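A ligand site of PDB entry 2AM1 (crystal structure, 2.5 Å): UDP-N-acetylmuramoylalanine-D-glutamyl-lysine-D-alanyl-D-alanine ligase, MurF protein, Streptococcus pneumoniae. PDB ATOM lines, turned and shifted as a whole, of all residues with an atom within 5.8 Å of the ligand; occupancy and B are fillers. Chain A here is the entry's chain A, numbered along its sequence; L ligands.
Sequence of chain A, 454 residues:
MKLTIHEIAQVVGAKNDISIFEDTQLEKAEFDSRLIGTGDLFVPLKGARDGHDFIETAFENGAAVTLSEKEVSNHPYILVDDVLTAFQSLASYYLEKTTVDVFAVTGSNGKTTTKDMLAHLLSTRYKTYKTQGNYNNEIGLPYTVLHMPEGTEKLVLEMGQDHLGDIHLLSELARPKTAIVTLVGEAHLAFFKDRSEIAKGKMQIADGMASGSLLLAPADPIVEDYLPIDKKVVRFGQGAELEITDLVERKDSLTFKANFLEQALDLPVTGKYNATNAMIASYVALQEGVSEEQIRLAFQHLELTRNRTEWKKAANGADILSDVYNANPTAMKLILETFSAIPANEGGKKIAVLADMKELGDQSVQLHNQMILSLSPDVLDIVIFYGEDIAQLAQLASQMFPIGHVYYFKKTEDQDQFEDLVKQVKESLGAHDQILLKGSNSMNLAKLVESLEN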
ATOM      1  N   PHE A  31     -12.473  -8.308 -11.260  1.00  0.00           N
ATOM      2  CA  PHE A  31     -12.127  -8.692  -9.883  1.00  0.00           C
ATOM      3  C   PHE A  31     -10.640  -8.399  -9.634  1.00  0.00           C
ATOM      4  O   PHE A  31     -10.135  -8.569  -8.530  1.00  0.00           O
ATOM      5  CB  PHE A  31     -12.413 -10.183  -9.597  1.00  0.00           C
ATOM      6  CG  PHE A  31     -11.753 -11.125 -10.562  1.00  0.00           C
ATOM      7  CD1 PHE A  31     -12.484 -11.679 -11.604  1.00  0.00           C
ATOM      8  CD2 PHE A  31     -10.402 -11.420 -10.446  1.00  0.00           C
ATOM      9  CE1 PHE A  31     -11.873 -12.525 -12.522  1.00  0.00           C
ATOM     10  CE2 PHE A  31      -9.791 -12.266 -11.363  1.00  0.00           C
ATOM     11  CZ  PHE A  31     -10.521 -12.820 -12.406  1.00  0.00           C
ATOM     12  N   ASP A  32      -9.959  -7.961 -10.684  1.00  0.00           N
ATOM     13  CA  ASP A  32      -8.548  -7.617 -10.626  1.00  0.00           C
ATOM     14  C   ASP A  32      -8.427  -6.092 -10.692  1.00  0.00           C
ATOM     15  O   ASP A  32      -8.420  -5.497 -11.789  1.00  0.00           O
ATOM     16  CB  ASP A  32      -7.792  -8.256 -11.809  1.00  0.00           C
ATOM     17  CG  ASP A  32      -6.301  -7.922 -11.820  1.00  0.00           C
ATOM     18  OD1 ASP A  32      -5.809  -7.285 -10.858  1.00  0.00           O
ATOM     19  OD2 ASP A  32      -5.612  -8.293 -12.790  1.00  0.00           O
ATOM     20  N   SER A  33      -8.344  -5.457  -9.524  1.00  0.00           N
ATOM     21  CA  SER A  33      -8.227  -3.999  -9.401  1.00  0.00           C
ATOM     22  C   SER A  33      -7.351  -3.408 -10.499  1.00  0.00           C
ATOM     23  O   SER A  33      -7.671  -2.392 -11.100  1.00  0.00           O
ATOM     24  CB  SER A  33      -7.626  -3.651  -8.041  1.00  0.00           C
ATOM     25  OG  SER A  33      -6.298  -4.158  -7.956  1.00  0.00           O
ATOM     26  N   ARG A  34      -6.245  -4.069 -10.744  1.00  0.00           N
ATOM     27  CA  ARG A  34      -5.265  -3.668 -11.734  1.00  0.00           C
ATOM     28  C   ARG A  34      -5.863  -3.643 -13.150  1.00  0.00           C
ATOM     29  O   ARG A  34      -5.202  -3.228 -14.103  1.00  0.00           O
ATOM     30  CB  ARG A  34      -4.097  -4.651 -11.629  1.00  0.00           C
ATOM     31  CG  ARG A  34      -2.995  -4.530 -12.643  1.00  0.00           C
ATOM     32  CD  ARG A  34      -1.971  -5.637 -12.402  1.00  0.00           C
ATOM     33  NE  ARG A  34      -2.614  -6.940 -12.239  1.00  0.00           N
ATOM     34  CZ  ARG A  34      -1.993  -8.120 -12.350  1.00  0.00           C
ATOM     35  NH1 ARG A  34      -0.698  -8.163 -12.636  1.00  0.00           N
ATOM     36  NH2 ARG A  34      -2.664  -9.247 -12.173  1.00  0.00           N
ATOM     37  N   LEU A  45     -13.018 -10.383  -4.495  1.00  0.00           N
ATOM     38  CA  LEU A  45     -13.094 -11.798  -4.157  1.00  0.00           C
ATOM     39  C   LEU A  45     -11.973 -12.265  -3.251  1.00  0.00           C
ATOM     40  O   LEU A  45     -10.950 -11.592  -3.122  1.00  0.00           O
ATOM     41  CB  LEU A  45     -13.085 -12.643  -5.431  1.00  0.00           C
ATOM     42  CG  LEU A  45     -14.187 -12.322  -6.441  1.00  0.00           C
ATOM     43  CD1 LEU A  45     -13.878 -13.007  -7.748  1.00  0.00           C
ATOM     44  CD2 LEU A  45     -15.538 -12.757  -5.878  1.00  0.00           C
ATOM     45  N   LYS A  46     -12.181 -13.420  -2.617  1.00  0.00           N
ATOM     46  CA  LYS A  46     -11.172 -14.016  -1.752  1.00  0.00           C
ATOM     47  C   LYS A  46     -10.111 -14.672  -2.630  1.00  0.00           C
ATOM     48  O   LYS A  46     -10.367 -15.723  -3.191  1.00  0.00           O
ATOM     49  CB  LYS A  46     -11.782 -15.096  -0.848  1.00  0.00           C
ATOM     50  CG  LYS A  46     -12.859 -14.620   0.112  1.00  0.00           C
ATOM     51  CD  LYS A  46     -13.213 -15.727   1.101  1.00  0.00           C
ATOM     52  CE  LYS A  46     -14.218 -15.283   2.160  1.00  0.00           C
ATOM     53  NZ  LYS A  46     -15.599 -15.166   1.639  1.00  0.00           N
ATOM     54  N   GLY A  47      -8.945 -14.054  -2.767  1.00  0.00           N
ATOM     55  CA  GLY A  47      -7.896 -14.628  -3.583  1.00  0.00           C
ATOM     56  C   GLY A  47      -6.661 -14.831  -2.731  1.00  0.00           C
ATOM     57  O   GLY A  47      -6.766 -15.293  -1.592  1.00  0.00           O
ATOM     58  N   ALA A  48      -5.486 -14.500  -3.262  1.00  0.00           N
ATOM     59  CA  ALA A  48      -4.253 -14.612  -2.488  1.00  0.00           C
ATOM     60  C   ALA A  48      -4.501 -13.716  -1.286  1.00  0.00           C
ATOM     61  O   ALA A  48      -4.144 -14.030  -0.147  1.00  0.00           O
ATOM     62  CB  ALA A  48      -3.071 -14.111  -3.305  1.00  0.00           C
ATOM     63  N   ARG A  49      -5.133 -12.585  -1.552  1.00  0.00           N
ATOM     64  CA  ARG A  49      -5.491 -11.640  -0.525  1.00  0.00           C
ATOM     65  C   ARG A  49      -6.962 -11.329  -0.748  1.00  0.00           C
ATOM     66  O   ARG A  49      -7.490 -11.575  -1.832  1.00  0.00           O
ATOM     67  CB  ARG A  49      -4.652 -10.371  -0.652  1.00  0.00           C
ATOM     68  CG  ARG A  49      -3.324 -10.485   0.044  1.00  0.00           C
ATOM     69  CD  ARG A  49      -2.550  -9.191  -0.010  1.00  0.00           C
ATOM     70  NE  ARG A  49      -1.741  -9.045   1.189  1.00  0.00           N
ATOM     71  CZ  ARG A  49      -2.212  -8.644   2.361  1.00  0.00           C
ATOM     72  NH1 ARG A  49      -3.500  -8.348   2.497  1.00  0.00           N
ATOM     73  NH2 ARG A  49      -1.410  -8.577   3.405  1.00  0.00           N
ATOM     74  N   ASP A  50      -7.627 -10.801   0.271  1.00  0.00           N
ATOM     75  CA  ASP A  50      -9.024 -10.484   0.068  1.00  0.00           C
ATOM     76  C   ASP A  50      -9.130  -9.307  -0.881  1.00  0.00           C
ATOM     77  O   ASP A  50      -8.386  -8.332  -0.770  1.00  0.00           O
ATOM     78  CB  ASP A  50      -9.703 -10.144   1.381  1.00  0.00           C
ATOM     79  CG  ASP A  50     -11.166  -9.923   1.196  1.00  0.00           C
ATOM     80  OD1 ASP A  50     -11.962 -10.771   1.659  1.00  0.00           O
ATOM     81  OD2 ASP A  50     -11.535  -8.909   0.558  1.00  0.00           O
ATOM     82  N   PHE A  54      -8.349  -4.077  -1.924  1.00  0.00           N
ATOM     83  CA  PHE A  54      -8.175  -3.274  -3.131  1.00  0.00           C
ATOM     84  C   PHE A  54      -9.319  -2.385  -3.590  1.00  0.00           C
ATOM     85  O   PHE A  54      -9.203  -1.725  -4.619  1.00  0.00           O
ATOM     86  CB  PHE A  54      -7.749  -4.189  -4.279  1.00  0.00           C
ATOM     87  CG  PHE A  54      -6.523  -4.977  -3.957  1.00  0.00           C
ATOM     88  CD1 PHE A  54      -6.558  -6.012  -3.032  1.00  0.00           C
ATOM     89  CD2 PHE A  54      -5.299  -4.637  -4.521  1.00  0.00           C
ATOM     90  CE1 PHE A  54      -5.414  -6.682  -2.677  1.00  0.00           C
ATOM     91  CE2 PHE A  54      -4.155  -5.307  -4.166  1.00  0.00           C
ATOM     92  CZ  PHE A  54      -4.206  -6.327  -3.242  1.00  0.00           C
ATOM     93  N   ASN A 134      -8.378 -20.237 -19.487  1.00  0.00           N
ATOM     94  CA  ASN A 134      -8.931 -21.308 -18.666  1.00  0.00           C
ATOM     95  C   ASN A 134      -9.916 -20.774 -17.621  1.00  0.00           C
ATOM     96  O   ASN A 134     -10.033 -21.314 -16.516  1.00  0.00           O
ATOM     97  CB  ASN A 134      -7.790 -22.048 -17.970  1.00  0.00           C
ATOM     98  CG  ASN A 134      -7.197 -21.260 -16.816  1.00  0.00           C
ATOM     99  OD1 ASN A 134      -7.270 -20.027 -16.789  1.00  0.00           O
ATOM    100  ND2 ASN A 134      -6.606 -21.960 -15.862  1.00  0.00           N
ATOM    101  N   TYR A 135     -10.613 -19.679 -17.969  1.00  0.00           N
ATOM    102  CA  TYR A 135     -11.597 -19.048 -17.091  1.00  0.00           C
ATOM    103  C   TYR A 135     -12.864 -19.895 -17.088  1.00  0.00           C
ATOM    104  O   TYR A 135     -13.937 -19.427 -17.452  1.00  0.00           O
ATOM    105  CB  TYR A 135     -11.938 -17.643 -17.599  1.00  0.00           C
ATOM    106  CG  TYR A 135     -11.035 -16.543 -17.077  1.00  0.00           C
ATOM    107  CD1 TYR A 135     -11.572 -15.319 -16.680  1.00  0.00           C
ATOM    108  CD2 TYR A 135      -9.659 -16.730 -16.954  1.00  0.00           C
ATOM    109  CE1 TYR A 135     -10.768 -14.325 -16.156  1.00  0.00           C
ATOM    110  CE2 TYR A 135      -8.845 -15.739 -16.438  1.00  0.00           C
ATOM    111  CZ  TYR A 135      -9.398 -14.531 -16.034  1.00  0.00           C
ATOM    112  OH  TYR A 135      -8.599 -13.547 -15.501  1.00  0.00           O
ATOM    113  N   ASN A 136     -12.740 -21.142 -16.634  1.00  0.00           N
ATOM    114  CA  ASN A 136     -13.849 -22.092 -16.644  1.00  0.00           C
ATOM    115  C   ASN A 136     -14.420 -22.569 -15.307  1.00  0.00           C
ATOM    116  O   ASN A 136     -15.013 -23.636 -15.259  1.00  0.00           O
ATOM    117  CB  ASN A 136     -13.414 -23.324 -17.439  1.00  0.00           C
ATOM    118  CG  ASN A 136     -12.324 -24.122 -16.732  1.00  0.00           C
ATOM    119  OD1 ASN A 136     -11.934 -23.770 -15.623  1.00  0.00           O
ATOM    120  ND2 ASN A 136     -11.842 -25.182 -17.363  1.00  0.00           N
ATOM    121  N   ASN A 137     -14.225 -21.825 -14.230  1.00  0.00           N
ATOM    122  CA  ASN A 137     -14.766 -22.264 -12.948  1.00  0.00           C
ATOM    123  C   ASN A 137     -15.807 -21.291 -12.409  1.00  0.00           C
ATOM    124  O   ASN A 137     -16.319 -20.465 -13.156  1.00  0.00           O
ATOM    125  CB  ASN A 137     -13.658 -22.495 -11.914  1.00  0.00           C
ATOM    126  CG  ASN A 137     -12.834 -21.236 -11.609  1.00  0.00           C
ATOM    127  OD1 ASN A 137     -13.156 -20.119 -12.015  1.00  0.00           O
ATOM    128  ND2 ASN A 137     -11.761 -21.430 -10.871  1.00  0.00           N
ATOM    129  N   ILE A 139     -15.544 -18.677 -10.917  1.00  0.00           N
ATOM    130  CA  ILE A 139     -15.169 -17.270 -11.043  1.00  0.00           C
ATOM    131  C   ILE A 139     -15.073 -16.912 -12.542  1.00  0.00           C
ATOM    132  O   ILE A 139     -15.604 -15.895 -12.980  1.00  0.00           O
ATOM    133  CB  ILE A 139     -13.776 -16.949 -10.392  1.00  0.00           C
ATOM    134  CG1 ILE A 139     -13.855 -16.924  -8.866  1.00  0.00           C
ATOM    135  CG2 ILE A 139     -13.310 -15.594 -10.871  1.00  0.00           C
ATOM    136  CD1 ILE A 139     -14.150 -18.260  -8.262  1.00  0.00           C
ATOM    137  N   GLY A 140     -14.395 -17.783 -13.299  1.00  0.00           N
ATOM    138  CA  GLY A 140     -14.182 -17.585 -14.717  1.00  0.00           C
ATOM    139  C   GLY A 140     -15.411 -17.561 -15.594  1.00  0.00           C
ATOM    140  O   GLY A 140     -15.563 -16.673 -16.430  1.00  0.00           O
ATOM    141  N   LEU A 141     -16.296 -18.535 -15.422  1.00  0.00           N
ATOM    142  CA  LEU A 141     -17.513 -18.573 -16.219  1.00  0.00           C
ATOM    143  C   LEU A 141     -18.325 -17.289 -16.000  1.00  0.00           C
ATOM    144  O   LEU A 141     -18.649 -16.579 -16.947  1.00  0.00           O
ATOM    145  CB  LEU A 141     -18.312 -19.831 -15.874  1.00  0.00           C
ATOM    146  CG  LEU A 141     -19.472 -20.194 -16.797  1.00  0.00           C
ATOM    147  CD1 LEU A 141     -19.632 -21.697 -16.858  1.00  0.00           C
ATOM    148  CD2 LEU A 141     -20.733 -19.502 -16.340  1.00  0.00           C
ATOM    149  N   ASN A 326      -1.751 -17.363 -16.382  1.00  0.00           N
ATOM    150  CA  ASN A 326      -2.347 -16.982 -15.116  1.00  0.00           C
ATOM    151  C   ASN A 326      -1.244 -16.661 -14.112  1.00  0.00           C
ATOM    152  O   ASN A 326      -1.181 -17.245 -13.034  1.00  0.00           O
ATOM    153  CB  ASN A 326      -3.250 -18.096 -14.588  1.00  0.00           C
ATOM    154  CG  ASN A 326      -4.700 -17.924 -14.996  1.00  0.00           C
ATOM    155  OD1 ASN A 326      -5.010 -17.328 -16.026  1.00  0.00           O
ATOM    156  ND2 ASN A 326      -5.608 -18.469 -14.193  1.00  0.00           N
ATOM    157  N   ASN A 328      -0.515 -14.731 -11.632  1.00  0.00           N
ATOM    158  CA  ASN A 328      -0.936 -13.855 -10.545  1.00  0.00           C
ATOM    159  C   ASN A 328      -0.918 -14.653  -9.250  1.00  0.00           C
ATOM    160  O   ASN A 328      -0.928 -15.871  -9.258  1.00  0.00           O
ATOM    161  CB  ASN A 328      -2.333 -13.247 -10.827  1.00  0.00           C
ATOM    162  CG  ASN A 328      -3.469 -14.274 -10.823  1.00  0.00           C
ATOM    163  OD1 ASN A 328      -4.024 -14.625  -9.782  1.00  0.00           O
ATOM    164  ND2 ASN A 328      -3.813 -14.771 -12.002  1.00  0.00           N
ATOM    165  N   PRO A 329      -0.879 -13.971  -8.107  1.00  0.00           N
ATOM    166  CA  PRO A 329      -0.849 -14.636  -6.815  1.00  0.00           C
ATOM    167  C   PRO A 329      -1.945 -15.648  -6.501  1.00  0.00           C
ATOM    168  O   PRO A 329      -1.678 -16.682  -5.868  1.00  0.00           O
ATOM    169  CB  PRO A 329      -0.792 -13.473  -5.822  1.00  0.00           C
ATOM    170  CG  PRO A 329      -1.413 -12.360  -6.552  1.00  0.00           C
ATOM    171  CD  PRO A 329      -0.862 -12.505  -7.936  1.00  0.00           C
ATOM    172  N   THR A 330      -3.179 -15.366  -6.915  1.00  0.00           N
ATOM    173  CA  THR A 330      -4.273 -16.292  -6.638  1.00  0.00           C
ATOM    174  C   THR A 330      -4.079 -17.575  -7.419  1.00  0.00           C
ATOM    175  O   THR A 330      -4.200 -18.665  -6.882  1.00  0.00           O
ATOM    176  CB  THR A 330      -5.641 -15.696  -7.018  1.00  0.00           C
ATOM    177  OG1 THR A 330      -5.832 -14.448  -6.350  1.00  0.00           O
ATOM    178  CG2 THR A 330      -6.753 -16.659  -6.614  1.00  0.00           C
ATOM    179  N   ALA A 331      -3.771 -17.420  -8.693  1.00  0.00           N
ATOM    180  CA  ALA A 331      -3.521 -18.542  -9.581  1.00  0.00           C
ATOM    181  C   ALA A 331      -2.411 -19.421  -8.996  1.00  0.00           C
ATOM    182  O   ALA A 331      -2.519 -20.640  -8.987  1.00  0.00           O
ATOM    183  CB  ALA A 331      -3.114 -18.031 -10.960  1.00  0.00           C
ATOM    184  N   LEU A 334      -3.595 -21.192  -5.945  1.00  0.00           N
ATOM    185  CA  LEU A 334      -4.494 -22.270  -6.355  1.00  0.00           C
ATOM    186  C   LEU A 334      -3.731 -23.442  -6.981  1.00  0.00           C
ATOM    187  O   LEU A 334      -4.016 -24.599  -6.671  1.00  0.00           O
ATOM    188  CB  LEU A 334      -5.566 -21.741  -7.322  1.00  0.00           C
ATOM    189  CG  LEU A 334      -6.578 -20.775  -6.688  1.00  0.00           C
ATOM    190  CD1 LEU A 334      -7.518 -20.238  -7.748  1.00  0.00           C
ATOM    191  CD2 LEU A 334      -7.345 -21.485  -5.580  1.00  0.00           C
ATOM    192  N   GLU A 359       4.854  -7.838 -13.234  1.00  0.00           N
ATOM    193  CA  GLU A 359       3.719  -6.923 -13.276  1.00  0.00           C
ATOM    194  C   GLU A 359       2.690  -7.012 -12.170  1.00  0.00           C
ATOM    195  O   GLU A 359       1.503  -6.812 -12.408  1.00  0.00           O
ATOM    196  CB  GLU A 359       3.030  -7.053 -14.630  1.00  0.00           C
ATOM    197  CG  GLU A 359       3.917  -6.609 -15.782  1.00  0.00           C
ATOM    198  CD  GLU A 359       3.445  -7.136 -17.121  1.00  0.00           C
ATOM    199  OE1 GLU A 359       2.247  -6.968 -17.443  1.00  0.00           O
ATOM    200  OE2 GLU A 359       4.276  -7.699 -17.866  1.00  0.00           O
ATOM    201  N   LEU A 360       3.109  -7.301 -10.951  1.00  0.00           N
ATOM    202  CA  LEU A 360       2.144  -7.366  -9.865  1.00  0.00           C
ATOM    203  C   LEU A 360       1.955  -5.984  -9.292  1.00  0.00           C
ATOM    204  O   LEU A 360       1.020  -5.737  -8.544  1.00  0.00           O
ATOM    205  CB  LEU A 360       2.614  -8.314  -8.765  1.00  0.00           C
ATOM    206  CG  LEU A 360       2.427  -9.798  -9.071  1.00  0.00           C
ATOM    207  CD1 LEU A 360       2.564 -10.583  -7.769  1.00  0.00           C
ATOM    208  CD2 LEU A 360       1.038 -10.029  -9.687  1.00  0.00           C
ATOM    209  N   GLY A 361       2.855  -5.073  -9.657  1.00  0.00           N
ATOM    210  CA  GLY A 361       2.763  -3.716  -9.152  1.00  0.00           C
ATOM    211  C   GLY A 361       3.717  -3.474  -8.010  1.00  0.00           C
ATOM    212  O   GLY A 361       4.551  -4.326  -7.694  1.00  0.00           O
ATOM    213  N   GLN A 363       3.318  -3.824  -5.189  1.00  0.00           N
ATOM    214  CA  GLN A 363       3.049  -4.766  -4.101  1.00  0.00           C
ATOM    215  C   GLN A 363       3.600  -6.170  -4.412  1.00  0.00           C
ATOM    216  O   GLN A 363       3.440  -7.091  -3.621  1.00  0.00           O
ATOM    217  CB  GLN A 363       1.543  -4.831  -3.849  1.00  0.00           C
ATOM    218  CG  GLN A 363       1.153  -4.776  -2.385  1.00  0.00           C
ATOM    219  CD  GLN A 363       1.595  -3.476  -1.728  1.00  0.00           C
ATOM    220  OE1 GLN A 363       2.780  -3.153  -1.692  1.00  0.00           O
ATOM    221  NE2 GLN A 363       0.638  -2.730  -1.186  1.00  0.00           N
ATOM    222  N   LEU A 367       3.267  -9.751  -2.253  1.00  0.00           N
ATOM    223  CA  LEU A 367       2.388 -10.761  -2.809  1.00  0.00           C
ATOM    224  C   LEU A 367       3.086 -12.100  -2.945  1.00  0.00           C
ATOM    225  O   LEU A 367       2.466 -13.147  -2.789  1.00  0.00           O
ATOM    226  CB  LEU A 367       1.846 -10.285  -4.159  1.00  0.00           C
ATOM    227  CG  LEU A 367       1.059  -8.982  -4.006  1.00  0.00           C
ATOM    228  CD1 LEU A 367       0.755  -8.371  -5.369  1.00  0.00           C
ATOM    229  CD2 LEU A 367      -0.200  -9.245  -3.212  1.00  0.00           C
HETATM  230  C1  LIG L   1      -2.871  -8.822  -5.982  1.00  0.00           C
HETATM  231  C2  LIG L   1      -5.117 -11.203  -7.963  1.00  0.00           C
HETATM  232  C3  LIG L   1      -4.805 -11.190  -5.525  1.00  0.00           C
HETATM  233  C4  LIG L   1      -2.562  -8.036  -8.889  1.00  0.00           C
HETATM  234  C5  LIG L   1      -6.600 -12.627  -9.185  1.00  0.00           C
HETATM  235  C6  LIG L   1      -8.648 -13.912  -8.267  1.00  0.00           C
HETATM  236  C7  LIG L   1      -9.077 -16.173  -9.192  1.00  0.00           C
HETATM  237  C8  LIG L   1      -8.559 -18.881 -13.075  1.00  0.00           C
HETATM  238  C9  LIG L   1      -3.603  -9.537  -7.102  1.00  0.00           C
HETATM  239  C10 LIG L   1      -4.543 -10.679  -6.853  1.00  0.00           C
HETATM  240  C11 LIG L   1      -3.460  -9.167  -8.432  1.00  0.00           C
HETATM  241  S1  LIG L   1      -4.499 -10.276  -9.327  1.00  0.00           S
HETATM  242  C12 LIG L   1      -2.460  -7.374  -6.364  1.00  0.00           C
HETATM  243  N1  LIG L   1      -5.994 -12.244  -8.025  1.00  0.00           N
HETATM  244  N2  LIG L   1      -5.021 -11.599  -4.469  1.00  0.00           N
HETATM  245  C13 LIG L   1      -1.734  -7.343  -7.747  1.00  0.00           C
HETATM  246  C14 LIG L   1      -7.503 -13.796  -9.134  1.00  0.00           C
HETATM  247  O1  LIG L   1      -6.390 -12.056 -10.275  1.00  0.00           O
HETATM  248  C15 LIG L   1      -7.181 -14.859 -10.009  1.00  0.00           C
HETATM  249  C16 LIG L   1      -7.943 -16.023 -10.049  1.00  0.00           C
HETATM  250  C17 LIG L   1      -9.433 -15.112  -8.301  1.00  0.00           C
HETATM  251 CL1  LIG L   1      -9.108 -12.644  -7.181  1.00  0.00          CL
HETATM  252  S2  LIG L   1      -7.456 -17.335 -11.214  1.00  0.00           S
HETATM  253  N3  LIG L   1      -8.878 -17.783 -12.127  1.00  0.00           N
HETATM  254  O2  LIG L   1      -6.995 -18.482 -10.477  1.00  0.00           O
HETATM  255  O3  LIG L   1      -6.416 -16.868 -12.092  1.00  0.00           O
HETATM  256 CL2  LIG L   1     -10.027 -17.646  -9.230  1.00  0.00          CL
HETATM  257  C18 LIG L   1      -9.382 -16.611 -12.879  1.00  0.00           C
HETATM  258  C19 LIG L   1     -10.656 -17.011 -13.668  1.00  0.00           C
HETATM  259  C20 LIG L   1      -9.821 -19.283 -13.882  1.00  0.00           C
HETATM  260  O4  LIG L   1     -10.939 -18.427 -13.540  1.00  0.00           O
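The side-chain amide nitrogen (ND2) of Asn 326 is in hydrogen-bond range of an oxygen (O3) of the ligand, 2.8 Å away. NH2 of Arg 34 lies close to S1 of the ligand (3.5 Å). N of Ala 48 lies within hydrogen-bond range of N2 of the ligand (3.2 Å). N of Arg 49 sits at hydrogen-bond distance from N2 of the ligand. The side-chain hydroxyl (OG1) of Thr 330 is in hydrogen-bond range of a nitrogen (N1) of the ligand, at 2.8 Å. The side-chain amide oxygen (OD1) of Asn 137 sits close to an oxygen (O4) of the ligand (3.2 Å). An oxygen (O3) of the ligand lies within hydrogen-bond range of the side-chain amide nitrogen (ND2) of Asn 328, at 3.3 Å.
OD2 of Asp 32 is in salt-bridge range of NH2 of Arg 34 (3.2 Å). The backbone NH of Gly 140 lies within hydrogen-bond range of the side-chain amide oxygen of Asn 137 (2.9 Å). N of Thr 330 is in hydrogen-bond range of OD1 of Asn 328 (3.1 Å). The backbone carbonyl oxygen of Tyr 135 sits at hydrogen-bond distance from the backbone NH of Leu 141, 3.2 Å away. The backbone carbonyl oxygen of Asn 134 lies close to the side-chain amide oxygen of Asn 136, 3.2 Å away. OD1 of Asn 328 is in hydrogen-bond range of N of Ala 331, 3.0 Å away. NH1 of Arg 34 sits at hydrogen-bond distance from O of Glu 359, 2.6 Å away. The backbone NH of Ala 48 lies within hydrogen-bond range of the side-chain hydroxyl of Thr 330 (3.1 Å).
The side-chain carboxylate (OD1) of Asp 32 lies close to a sulfur (S1) of the ligand, 3.6 Å away. Phe 31 touches the ligand (CE2 to C14, 3.5 Å). Phe 54 touches the ligand. O of Asn 134 touches C20 of the ligand, 3.3 Å away. CD2 of Tyr 135 touches C19 of the ligand, 3.4 Å away. CG1 of Ile 139 touches CL2 of the ligand, at 3.9 Å. Gly 140 touches the ligand (N to O4, 3.5 Å). CG of Pro 329 touches C10 of the ligand, at 3.6 Å. CA of Ala 331 touches O2 of the ligand, 3.6 Å away. Leu 334 touches the ligand (CD1 to O2, 3.3 Å). O of Leu 360 touches C13 of the ligand (3.3 Å). CD1 of Leu 367 touches C12 of the ligand (3.5 Å). Hydrophobic or aromatic side chains that line the ligand: Phe 31, Ala 48, Phe 54, Tyr 135, Ile 139, Pro 329, Ala 331, Leu 334 and Leu 367. Within 4 Å of the ligand: Phe 31, Asp 32, Arg 34, Ala 48, Arg 49, Phe 54, Asn 134, Tyr 135, Asn 137, Ile 139, Gly 140, Asn 326, Asn 328, Pro 329, Thr 330, Ala 331, Leu 334, Leu 360 and Leu 367.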
